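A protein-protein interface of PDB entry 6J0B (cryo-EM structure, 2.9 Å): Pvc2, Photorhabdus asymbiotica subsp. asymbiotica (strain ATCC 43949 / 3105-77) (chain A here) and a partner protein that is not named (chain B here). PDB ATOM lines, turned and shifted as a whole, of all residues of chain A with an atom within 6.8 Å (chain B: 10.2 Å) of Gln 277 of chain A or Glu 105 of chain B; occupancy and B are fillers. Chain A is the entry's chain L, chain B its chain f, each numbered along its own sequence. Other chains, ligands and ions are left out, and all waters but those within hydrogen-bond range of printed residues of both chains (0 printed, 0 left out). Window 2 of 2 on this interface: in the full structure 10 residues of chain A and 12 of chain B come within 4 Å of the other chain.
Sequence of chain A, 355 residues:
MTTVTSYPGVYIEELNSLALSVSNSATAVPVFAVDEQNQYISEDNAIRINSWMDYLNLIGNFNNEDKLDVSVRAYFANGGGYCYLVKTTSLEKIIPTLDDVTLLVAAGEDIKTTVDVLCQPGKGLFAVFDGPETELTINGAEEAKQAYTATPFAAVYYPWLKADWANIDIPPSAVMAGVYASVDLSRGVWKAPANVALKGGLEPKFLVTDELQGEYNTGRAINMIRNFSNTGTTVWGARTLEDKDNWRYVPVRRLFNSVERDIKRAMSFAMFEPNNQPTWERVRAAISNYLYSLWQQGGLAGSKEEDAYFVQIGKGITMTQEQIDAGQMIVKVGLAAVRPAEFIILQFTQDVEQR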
ATOM      1  N   PRO A 274       6.565  24.692  29.053  1.00  0.00           N
ATOM      2  CA  PRO A 274       7.865  24.029  29.237  1.00  0.00           C
ATOM      3  C   PRO A 274       8.981  24.733  28.479  1.00  0.00           C
ATOM      4  O   PRO A 274       8.813  25.148  27.332  1.00  0.00           O
ATOM      5  CB  PRO A 274       7.620  22.617  28.693  1.00  0.00           C
ATOM      6  CG  PRO A 274       6.372  22.717  27.891  1.00  0.00           C
ATOM      7  CD  PRO A 274       5.552  23.716  28.615  1.00  0.00           C
ATOM      8  N   ASN A 275      10.122  24.877  29.145  1.00  0.00           N
ATOM      9  CA  ASN A 275      11.261  25.609  28.597  1.00  0.00           C
ATOM     10  C   ASN A 275      12.109  24.638  27.793  1.00  0.00           C
ATOM     11  O   ASN A 275      13.103  24.098  28.276  1.00  0.00           O
ATOM     12  CB  ASN A 275      12.063  26.265  29.711  1.00  0.00           C
ATOM     13  CG  ASN A 275      12.861  27.448  29.229  1.00  0.00           C
ATOM     14  OD1 ASN A 275      12.682  27.913  28.108  1.00  0.00           O
ATOM     15  ND2 ASN A 275      13.741  27.952  30.077  1.00  0.00           N
ATOM     16  N   ASN A 276      11.706  24.407  26.550  1.00  0.00           N
ATOM     17  CA  ASN A 276      12.454  23.557  25.640  1.00  0.00           C
ATOM     18  C   ASN A 276      12.414  24.199  24.261  1.00  0.00           C
ATOM     19  O   ASN A 276      11.941  25.326  24.098  1.00  0.00           O
ATOM     20  CB  ASN A 276      11.896  22.129  25.641  1.00  0.00           C
ATOM     21  CG  ASN A 276      10.388  22.088  25.521  1.00  0.00           C
ATOM     22  OD1 ASN A 276       9.734  23.120  25.395  1.00  0.00           O
ATOM     23  ND2 ASN A 276       9.826  20.888  25.556  1.00  0.00           N
ATOM     24  N   GLN A 277      12.911  23.482  23.268  1.00  0.00           N
ATOM     25  CA  GLN A 277      12.936  24.003  21.905  1.00  0.00           C
ATOM     26  C   GLN A 277      11.572  24.163  21.221  1.00  0.00           C
ATOM     27  O   GLN A 277      11.420  25.145  20.487  1.00  0.00           O
ATOM     28  CB  GLN A 277      13.848  23.148  21.022  1.00  0.00           C
ATOM     29  CG  GLN A 277      14.327  23.901  19.804  1.00  0.00           C
ATOM     30  CD  GLN A 277      15.034  23.032  18.814  1.00  0.00           C
ATOM     31  OE1 GLN A 277      14.714  21.862  18.660  1.00  0.00           O
ATOM     32  NE2 GLN A 277      16.007  23.602  18.127  1.00  0.00           N
ATOM     33  N   PRO A 278      10.565  23.279  21.388  1.00  0.00           N
ATOM     34  CA  PRO A 278       9.267  23.567  20.743  1.00  0.00           C
ATOM     35  C   PRO A 278       8.551  24.808  21.254  1.00  0.00           C
ATOM     36  O   PRO A 278       7.675  25.327  20.555  1.00  0.00           O
ATOM     37  CB  PRO A 278       8.446  22.299  21.020  1.00  0.00           C
ATOM     38  CG  PRO A 278       9.150  21.612  22.104  1.00  0.00           C
ATOM     39  CD  PRO A 278      10.572  21.870  21.829  1.00  0.00           C
ATOM     40  N   THR A 279       8.900  25.309  22.438  1.00  0.00           N
ATOM     41  CA  THR A 279       8.372  26.598  22.864  1.00  0.00           C
ATOM     42  C   THR A 279       9.093  27.741  22.160  1.00  0.00           C
ATOM     43  O   THR A 279       8.449  28.680  21.679  1.00  0.00           O
ATOM     44  CB  THR A 279       8.483  26.729  24.381  1.00  0.00           C
ATOM     45  OG1 THR A 279       7.689  25.712  24.999  1.00  0.00           O
ATOM     46  CG2 THR A 279       7.991  28.083  24.853  1.00  0.00           C
ATOM     47  N   TRP A 280      10.424  27.653  22.049  1.00  0.00           N
ATOM     48  CA  TRP A 280      11.225  28.739  21.486  1.00  0.00           C
ATOM     49  C   TRP A 280      10.948  28.958  20.008  1.00  0.00           C
ATOM     50  O   TRP A 280      11.050  30.087  19.522  1.00  0.00           O
ATOM     51  CB  TRP A 280      12.711  28.454  21.671  1.00  0.00           C
ATOM     52  CG  TRP A 280      13.128  28.216  23.070  1.00  0.00           C
ATOM     53  CD1 TRP A 280      12.527  28.680  24.195  1.00  0.00           C
ATOM     54  CD2 TRP A 280      14.249  27.444  23.500  1.00  0.00           C
ATOM     55  NE1 TRP A 280      13.204  28.247  25.305  1.00  0.00           N
ATOM     56  CE2 TRP A 280      14.267  27.484  24.903  1.00  0.00           C
ATOM     57  CE3 TRP A 280      15.239  26.720  22.834  1.00  0.00           C
ATOM     58  CZ2 TRP A 280      15.235  26.829  25.652  1.00  0.00           C
ATOM     59  CZ3 TRP A 280      16.198  26.071  23.578  1.00  0.00           C
ATOM     60  CH2 TRP A 280      16.191  26.129  24.971  1.00  0.00           C
ATOM     61  N   GLU A 281      10.603  27.906  19.277  1.00  0.00           N
ATOM     62  CA  GLU A 281      10.249  28.079  17.879  1.00  0.00           C
ATOM     63  C   GLU A 281       8.812  28.530  17.697  1.00  0.00           C
ATOM     64  O   GLU A 281       8.413  28.839  16.572  1.00  0.00           O
ATOM     65  CB  GLU A 281      10.486  26.782  17.124  1.00  0.00           C
ATOM     66  CG  GLU A 281      11.828  26.158  17.434  1.00  0.00           C
ATOM     67  CD  GLU A 281      12.934  26.680  16.562  1.00  0.00           C
ATOM     68  OE1 GLU A 281      14.106  26.337  16.821  1.00  0.00           O
ATOM     69  OE2 GLU A 281      12.632  27.425  15.613  1.00  0.00           O
ATOM     70  N   ARG A 282       8.034  28.563  18.771  1.00  0.00           N
ATOM     71  CA  ARG A 282       6.722  29.184  18.754  1.00  0.00           C
ATOM     72  C   ARG A 282       6.779  30.623  19.231  1.00  0.00           C
ATOM     73  O   ARG A 282       5.959  31.444  18.808  1.00  0.00           O
ATOM     74  CB  ARG A 282       5.762  28.383  19.629  1.00  0.00           C
ATOM     75  CG  ARG A 282       4.325  28.496  19.223  1.00  0.00           C
ATOM     76  CD  ARG A 282       3.644  27.167  19.400  1.00  0.00           C
ATOM     77  NE  ARG A 282       3.666  26.720  20.786  1.00  0.00           N
ATOM     78  CZ  ARG A 282       2.665  26.895  21.640  1.00  0.00           C
ATOM     79  NH1 ARG A 282       1.558  27.509  21.247  1.00  0.00           N
ATOM     80  NH2 ARG A 282       2.770  26.455  22.886  1.00  0.00           N
ATOM     81  N   LYS A 315      19.634  27.836  22.102  1.00  0.00           N
ATOM     82  CA  LYS A 315      20.426  27.350  23.224  1.00  0.00           C
ATOM     83  C   LYS A 315      21.904  27.667  23.036  1.00  0.00           C
ATOM     84  O   LYS A 315      22.629  27.888  24.008  1.00  0.00           O
ATOM     85  CB  LYS A 315      20.212  25.847  23.399  1.00  0.00           C
ATOM     86  CG  LYS A 315      20.887  25.239  24.616  1.00  0.00           C
ATOM     87  CD  LYS A 315      20.671  23.745  24.666  1.00  0.00           C
ATOM     88  CE  LYS A 315      21.697  23.073  25.556  1.00  0.00           C
ATOM     89  NZ  LYS A 315      21.482  21.600  25.628  1.00  0.00           N
ATOM     90  N   ALA B   9      21.656  12.285  11.970  1.00  0.00           N
ATOM     91  CA  ALA B   9      20.970  13.529  12.292  1.00  0.00           C
ATOM     92  C   ALA B   9      21.373  14.678  11.379  1.00  0.00           C
ATOM     93  O   ALA B   9      20.626  15.654  11.271  1.00  0.00           O
ATOM     94  CB  ALA B   9      21.243  13.916  13.742  1.00  0.00           C
ATOM     95  N   ILE B  14      14.409  13.674   6.343  1.00  0.00           N
ATOM     96  CA  ILE B  14      13.511  13.719   7.494  1.00  0.00           C
ATOM     97  C   ILE B  14      12.216  13.004   7.130  1.00  0.00           C
ATOM     98  O   ILE B  14      11.617  13.329   6.097  1.00  0.00           O
ATOM     99  CB  ILE B  14      13.229  15.166   7.922  1.00  0.00           C
ATOM    100  CG1 ILE B  14      14.536  15.906   8.174  1.00  0.00           C
ATOM    101  CG2 ILE B  14      12.379  15.184   9.164  1.00  0.00           C
ATOM    102  CD1 ILE B  14      14.341  17.354   8.473  1.00  0.00           C
ATOM    103  N   ARG B  18       6.148  12.351  11.770  1.00  0.00           N
ATOM    104  CA  ARG B  18       6.254  12.894  13.117  1.00  0.00           C
ATOM    105  C   ARG B  18       6.275  14.413  13.022  1.00  0.00           C
ATOM    106  O   ARG B  18       7.266  14.996  12.578  1.00  0.00           O
ATOM    107  CB  ARG B  18       7.504  12.353  13.802  1.00  0.00           C
ATOM    108  CG  ARG B  18       7.510  12.433  15.314  1.00  0.00           C
ATOM    109  CD  ARG B  18       6.303  11.763  15.929  1.00  0.00           C
ATOM    110  NE  ARG B  18       6.058  10.427  15.401  1.00  0.00           N
ATOM    111  CZ  ARG B  18       6.227   9.311  16.094  1.00  0.00           C
ATOM    112  NH1 ARG B  18       6.646   9.369  17.348  1.00  0.00           N
ATOM    113  NH2 ARG B  18       5.977   8.138  15.534  1.00  0.00           N
ATOM    114  N   PHE B  19       5.179  15.052  13.430  1.00  0.00           N
ATOM    115  CA  PHE B  19       5.058  16.494  13.285  1.00  0.00           C
ATOM    116  C   PHE B  19       4.169  17.057  14.383  1.00  0.00           C
ATOM    117  O   PHE B  19       3.337  16.355  14.958  1.00  0.00           O
ATOM    118  CB  PHE B  19       4.528  16.883  11.897  1.00  0.00           C
ATOM    119  CG  PHE B  19       3.208  16.261  11.533  1.00  0.00           C
ATOM    120  CD1 PHE B  19       2.019  16.922  11.785  1.00  0.00           C
ATOM    121  CD2 PHE B  19       3.158  15.039  10.891  1.00  0.00           C
ATOM    122  CE1 PHE B  19       0.816  16.360  11.440  1.00  0.00           C
ATOM    123  CE2 PHE B  19       1.959  14.476  10.547  1.00  0.00           C
ATOM    124  CZ  PHE B  19       0.788  15.138  10.819  1.00  0.00           C
ATOM    125  N   ILE B  20       4.357  18.345  14.668  1.00  0.00           N
ATOM    126  CA  ILE B  20       3.576  19.074  15.660  1.00  0.00           C
ATOM    127  C   ILE B  20       2.875  20.227  14.960  1.00  0.00           C
ATOM    128  O   ILE B  20       3.525  21.037  14.294  1.00  0.00           O
ATOM    129  CB  ILE B  20       4.450  19.614  16.806  1.00  0.00           C
ATOM    130  CG1 ILE B  20       5.341  18.524  17.378  1.00  0.00           C
ATOM    131  CG2 ILE B  20       3.588  20.178  17.908  1.00  0.00           C
ATOM    132  CD1 ILE B  20       4.597  17.368  17.972  1.00  0.00           C
ATOM    133  N   THR B  95       1.655  26.686  12.961  1.00  0.00           N
ATOM    134  CA  THR B  95       3.028  26.251  12.748  1.00  0.00           C
ATOM    135  C   THR B  95       3.070  24.735  12.667  1.00  0.00           C
ATOM    136  O   THR B  95       2.622  24.053  13.589  1.00  0.00           O
ATOM    137  CB  THR B  95       3.968  26.715  13.866  1.00  0.00           C
ATOM    138  OG1 THR B  95       3.733  25.932  15.038  1.00  0.00           O
ATOM    139  CG2 THR B  95       3.768  28.185  14.199  1.00  0.00           C
ATOM    140  N   SER B  97       5.770  21.504  12.350  1.00  0.00           N
ATOM    141  CA  SER B  97       7.153  21.319  12.779  1.00  0.00           C
ATOM    142  C   SER B  97       7.479  19.835  12.805  1.00  0.00           C
ATOM    143  O   SER B  97       6.962  19.115  13.658  1.00  0.00           O
ATOM    144  CB  SER B  97       7.374  21.940  14.149  1.00  0.00           C
ATOM    145  OG  SER B  97       7.246  23.346  14.113  1.00  0.00           O
ATOM    146  N   LEU B  98       8.354  19.394  11.905  1.00  0.00           N
ATOM    147  CA  LEU B  98       8.850  18.026  11.938  1.00  0.00           C
ATOM    148  C   LEU B  98       9.753  17.824  13.148  1.00  0.00           C
ATOM    149  O   LEU B  98      10.687  18.597  13.369  1.00  0.00           O
ATOM    150  CB  LEU B  98       9.618  17.713  10.659  1.00  0.00           C
ATOM    151  CG  LEU B  98       8.838  17.665   9.352  1.00  0.00           C
ATOM    152  CD1 LEU B  98       9.786  17.757   8.182  1.00  0.00           C
ATOM    153  CD2 LEU B  98       8.041  16.391   9.273  1.00  0.00           C
ATOM    154  N   THR B  99       9.477  16.786  13.932  1.00  0.00           N
ATOM    155  CA  THR B  99      10.202  16.528  15.167  1.00  0.00           C
ATOM    156  C   THR B  99      10.800  15.131  15.159  1.00  0.00           C
ATOM    157  O   THR B  99      10.600  14.343  14.233  1.00  0.00           O
ATOM    158  CB  THR B  99       9.300  16.669  16.397  1.00  0.00           C
ATOM    159  OG1 THR B  99       8.147  15.837  16.248  1.00  0.00           O
ATOM    160  CG2 THR B  99       8.860  18.074  16.551  1.00  0.00           C
ATOM    161  N   ASN B 100      11.539  14.837  16.225  1.00  0.00           N
ATOM    162  CA  ASN B 100      12.043  13.502  16.489  1.00  0.00           C
ATOM    163  C   ASN B 100      11.003  12.703  17.268  1.00  0.00           C
ATOM    164  O   ASN B 100       9.892  13.169  17.525  1.00  0.00           O
ATOM    165  CB  ASN B 100      13.362  13.577  17.249  1.00  0.00           C
ATOM    166  CG  ASN B 100      13.260  14.420  18.496  1.00  0.00           C
ATOM    167  OD1 ASN B 100      12.365  15.246  18.617  1.00  0.00           O
ATOM    168  ND2 ASN B 100      14.178  14.219  19.429  1.00  0.00           N
ATOM    169  N   ASP B 101      11.364  11.479  17.643  1.00  0.00           N
ATOM    170  CA  ASP B 101      10.486  10.658  18.465  1.00  0.00           C
ATOM    171  C   ASP B 101      10.399  11.238  19.868  1.00  0.00           C
ATOM    172  O   ASP B 101      11.431  11.512  20.492  1.00  0.00           O
ATOM    173  CB  ASP B 101      10.998   9.222  18.519  1.00  0.00           C
ATOM    174  CG  ASP B 101      10.116   8.260  17.754  1.00  0.00           C
ATOM    175  OD1 ASP B 101       8.996   8.654  17.377  1.00  0.00           O
ATOM    176  OD2 ASP B 101      10.541   7.107  17.529  1.00  0.00           O
ATOM    177  N   ALA B 102       9.165  11.416  20.352  1.00  0.00           N
ATOM    178  CA  ALA B 102       8.842  12.103  21.606  1.00  0.00           C
ATOM    179  C   ALA B 102       9.449  13.506  21.614  1.00  0.00           C
ATOM    180  O   ALA B 102      10.396  13.806  22.341  1.00  0.00           O
ATOM    181  CB  ALA B 102       9.272  11.293  22.833  1.00  0.00           C
ATOM    182  N   GLY B 103       8.880  14.339  20.742  1.00  0.00           N
ATOM    183  CA  GLY B 103       9.493  15.567  20.273  1.00  0.00           C
ATOM    184  C   GLY B 103       9.895  16.596  21.304  1.00  0.00           C
ATOM    185  O   GLY B 103       9.064  17.314  21.866  1.00  0.00           O
ATOM    186  N   THR B 104      11.201  16.663  21.544  1.00  0.00           N
ATOM    187  CA  THR B 104      11.828  17.709  22.335  1.00  0.00           C
ATOM    188  C   THR B 104      12.764  18.543  21.477  1.00  0.00           C
ATOM    189  O   THR B 104      13.521  19.363  22.008  1.00  0.00           O
ATOM    190  CB  THR B 104      12.603  17.108  23.509  1.00  0.00           C
ATOM    191  OG1 THR B 104      13.667  16.292  23.005  1.00  0.00           O
ATOM    192  CG2 THR B 104      11.693  16.257  24.369  1.00  0.00           C
ATOM    193  N   GLU B 105      12.723  18.352  20.163  1.00  0.00           N
ATOM    194  CA  GLU B 105      13.723  18.908  19.262  1.00  0.00           C
ATOM    195  C   GLU B 105      13.089  19.013  17.889  1.00  0.00           C
ATOM    196  O   GLU B 105      12.632  18.004  17.348  1.00  0.00           O
ATOM    197  CB  GLU B 105      14.961  18.014  19.225  1.00  0.00           C
ATOM    198  CG  GLU B 105      16.262  18.735  18.955  1.00  0.00           C
ATOM    199  CD  GLU B 105      16.740  19.546  20.145  1.00  0.00           C
ATOM    200  OE1 GLU B 105      16.933  18.965  21.232  1.00  0.00           O
ATOM    201  OE2 GLU B 105      16.923  20.770  19.995  1.00  0.00           O
ATOM    202  N   LEU B 106      13.044  20.215  17.330  1.00  0.00           N
ATOM    203  CA  LEU B 106      12.460  20.412  16.014  1.00  0.00           C
ATOM    204  C   LEU B 106      13.533  20.260  14.949  1.00  0.00           C
ATOM    205  O   LEU B 106      14.693  20.622  15.163  1.00  0.00           O
ATOM    206  CB  LEU B 106      11.813  21.787  15.885  1.00  0.00           C
ATOM    207  CG  LEU B 106      10.861  22.388  16.915  1.00  0.00           C
ATOM    208  CD1 LEU B 106      10.076  23.421  16.206  1.00  0.00           C
ATOM    209  CD2 LEU B 106       9.907  21.414  17.513  1.00  0.00           C
ATOM    210  N   LEU B 107      13.140  19.733  13.797  1.00  0.00           N
ATOM    211  CA  LEU B 107      14.055  19.568  12.677  1.00  0.00           C
ATOM    212  C   LEU B 107      13.788  20.567  11.561  1.00  0.00           C
ATOM    213  O   LEU B 107      14.730  21.136  11.008  1.00  0.00           O
ATOM    214  CB  LEU B 107      13.961  18.140  12.134  1.00  0.00           C
ATOM    215  CG  LEU B 107      13.997  17.037  13.193  1.00  0.00           C
ATOM    216  CD1 LEU B 107      13.848  15.674  12.561  1.00  0.00           C
ATOM    217  CD2 LEU B 107      15.273  17.097  14.000  1.00  0.00           C
ATOM    218  N   MET B 108      12.521  20.789  11.230  1.00  0.00           N
ATOM    219  CA  MET B 108      12.101  21.808  10.284  1.00  0.00           C
ATOM    220  C   MET B 108      10.862  22.484  10.841  1.00  0.00           C
ATOM    221  O   MET B 108      10.196  21.951  11.725  1.00  0.00           O
ATOM    222  CB  MET B 108      11.800  21.217   8.908  1.00  0.00           C
ATOM    223  CG  MET B 108      13.006  21.049   8.035  1.00  0.00           C
ATOM    224  SD  MET B 108      13.674  22.636   7.537  1.00  0.00           S
ATOM    225  CE  MET B 108      15.309  22.116   7.061  1.00  0.00           C
ATOM    226  N   THR B 109      10.560  23.673  10.329  1.00  0.00           N
ATOM    227  CA  THR B 109       9.410  24.422  10.814  1.00  0.00           C
ATOM    228  C   THR B 109       8.815  25.225   9.670  1.00  0.00           C
ATOM    229  O   THR B 109       9.537  25.940   8.974  1.00  0.00           O
ATOM    230  CB  THR B 109       9.794  25.358  11.969  1.00  0.00           C
ATOM    231  OG1 THR B 109      10.377  24.604  13.035  1.00  0.00           O
ATOM    232  CG2 THR B 109       8.575  26.081  12.509  1.00  0.00           C
ATOM    233  N   GLN B 147      11.351  27.482   8.022  1.00  0.00           N
ATOM    234  CA  GLN B 147      12.463  27.823   8.895  1.00  0.00           C
ATOM    235  C   GLN B 147      13.308  26.592   9.171  1.00  0.00           C
ATOM    236  O   GLN B 147      12.779  25.507   9.419  1.00  0.00           O
ATOM    237  CB  GLN B 147      11.970  28.410  10.216  1.00  0.00           C
ATOM    238  CG  GLN B 147      11.810  29.913  10.213  1.00  0.00           C
ATOM    239  CD  GLN B 147      13.109  30.640  10.504  1.00  0.00           C
ATOM    240  OE1 GLN B 147      14.152  30.018  10.706  1.00  0.00           O
ATOM    241  NE2 GLN B 147      13.048  31.964  10.534  1.00  0.00           N
ATOM    242  N   ALA B 148      14.622  26.765   9.126  1.00  0.00           N
ATOM    243  CA  ALA B 148      15.523  25.681   9.481  1.00  0.00           C
ATOM    244  C   ALA B 148      15.598  25.552  10.994  1.00  0.00           C
ATOM    245  O   ALA B 148      15.926  26.518  11.691  1.00  0.00           O
ATOM    246  CB  ALA B 148      16.912  25.929   8.899  1.00  0.00           C
ATOM    247  N   VAL B 149      15.281  24.352  11.487  1.00  0.00           N
ATOM    248  CA  VAL B 149      15.287  23.978  12.907  1.00  0.00           C
ATOM    249  C   VAL B 149      14.416  24.893  13.765  1.00  0.00           C
ATOM    250  O   VAL B 149      13.192  24.899  13.637  1.00  0.00           O
ATOM    251  CB  VAL B 149      16.726  23.926  13.463  1.00  0.00           C
ATOM    252  CG1 VAL B 149      16.723  23.356  14.854  1.00  0.00           C
ATOM    253  CG2 VAL B 149      17.619  23.093  12.558  1.00  0.00           C
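The side-chain amide oxygen (OE1) of Gln 277 of chain A sits close to the side-chain carboxylate (OE2) of Glu 105 of chain B (2.8 Å). The side-chain amide oxygen (OE1) of Gln 277 of chain A is in hydrogen-bond range of the backbone NH (N) of Leu 106 of chain B (2.7 Å). The side-chain carboxylate (OE2) of Glu 281 of chain A sits close to the backbone carbonyl oxygen (O) of Val 149 of chain B (3.3 Å).
The side-chain amide oxygen of Asn 100 of chain B sits at hydrogen-bond distance from the backbone NH of Thr 104 of chain B, at 3.5 Å. The backbone carbonyl oxygen (O) of Glu 105 of chain B sits close to the side-chain amide oxygen (OD1) of Asn 100 of chain B. O of Leu 107 of chain B lies within hydrogen-bond range of N of Val 149 of chain B (3.3 Å). The backbone carbonyl oxygen (O) of Val 149 of chain B sits at hydrogen-bond distance from the side-chain hydroxyl (OG1) of Thr 109 of chain B.
Gln 277 of chain A touches Thr 104 of chain B. Gln 277 of chain A touches Val 149 of chain B (NE2 to CG1, 3.4 Å). Pro 278 of chain A touches Thr 104 of chain B. CD2 of Leu 106 of chain B touches CB of Pro 278 of chain A, 3.9 Å away. Leu 106 of chain B touches Glu 281 of chain A.
No residue of chain B comes within 4 Å of Asn 276 of chain A. Gln 277 of chain A touches four residues of chain B. Pro 278 of chain A touches just these residues of chain B: Thr 104 and Leu 106. No residue of chain B comes within 4 Å of Trp 280 of chain A. Printed residues of chain B within 4 Å of Glu 281 of chain A: Leu 106 and Val 149. Ala 9 of chain B touches none of the printed residues of chain A. Of the printed residues of chain A, Thr 104 of chain B touches Gln 277 (3.9 Å) and Pro 278 (3.9 Å). Of chain A, only Gln 277 comes within 4 Å of Glu 105 of chain B. Of the printed residues of chain A, Val 149 of chain B touches Gln 277 (3.4 Å) and Glu 281 (3.3 Å). The nearest printed residue of chain B that does not touch Glu 281 of chain A is Thr 109 of chain B (4.4 Å).
Printed residues of chain A that touch a printed residue of chain B: Gln 277, Pro 278 and Glu 281. Among the printed residues, 8 pairs touch across the chains.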
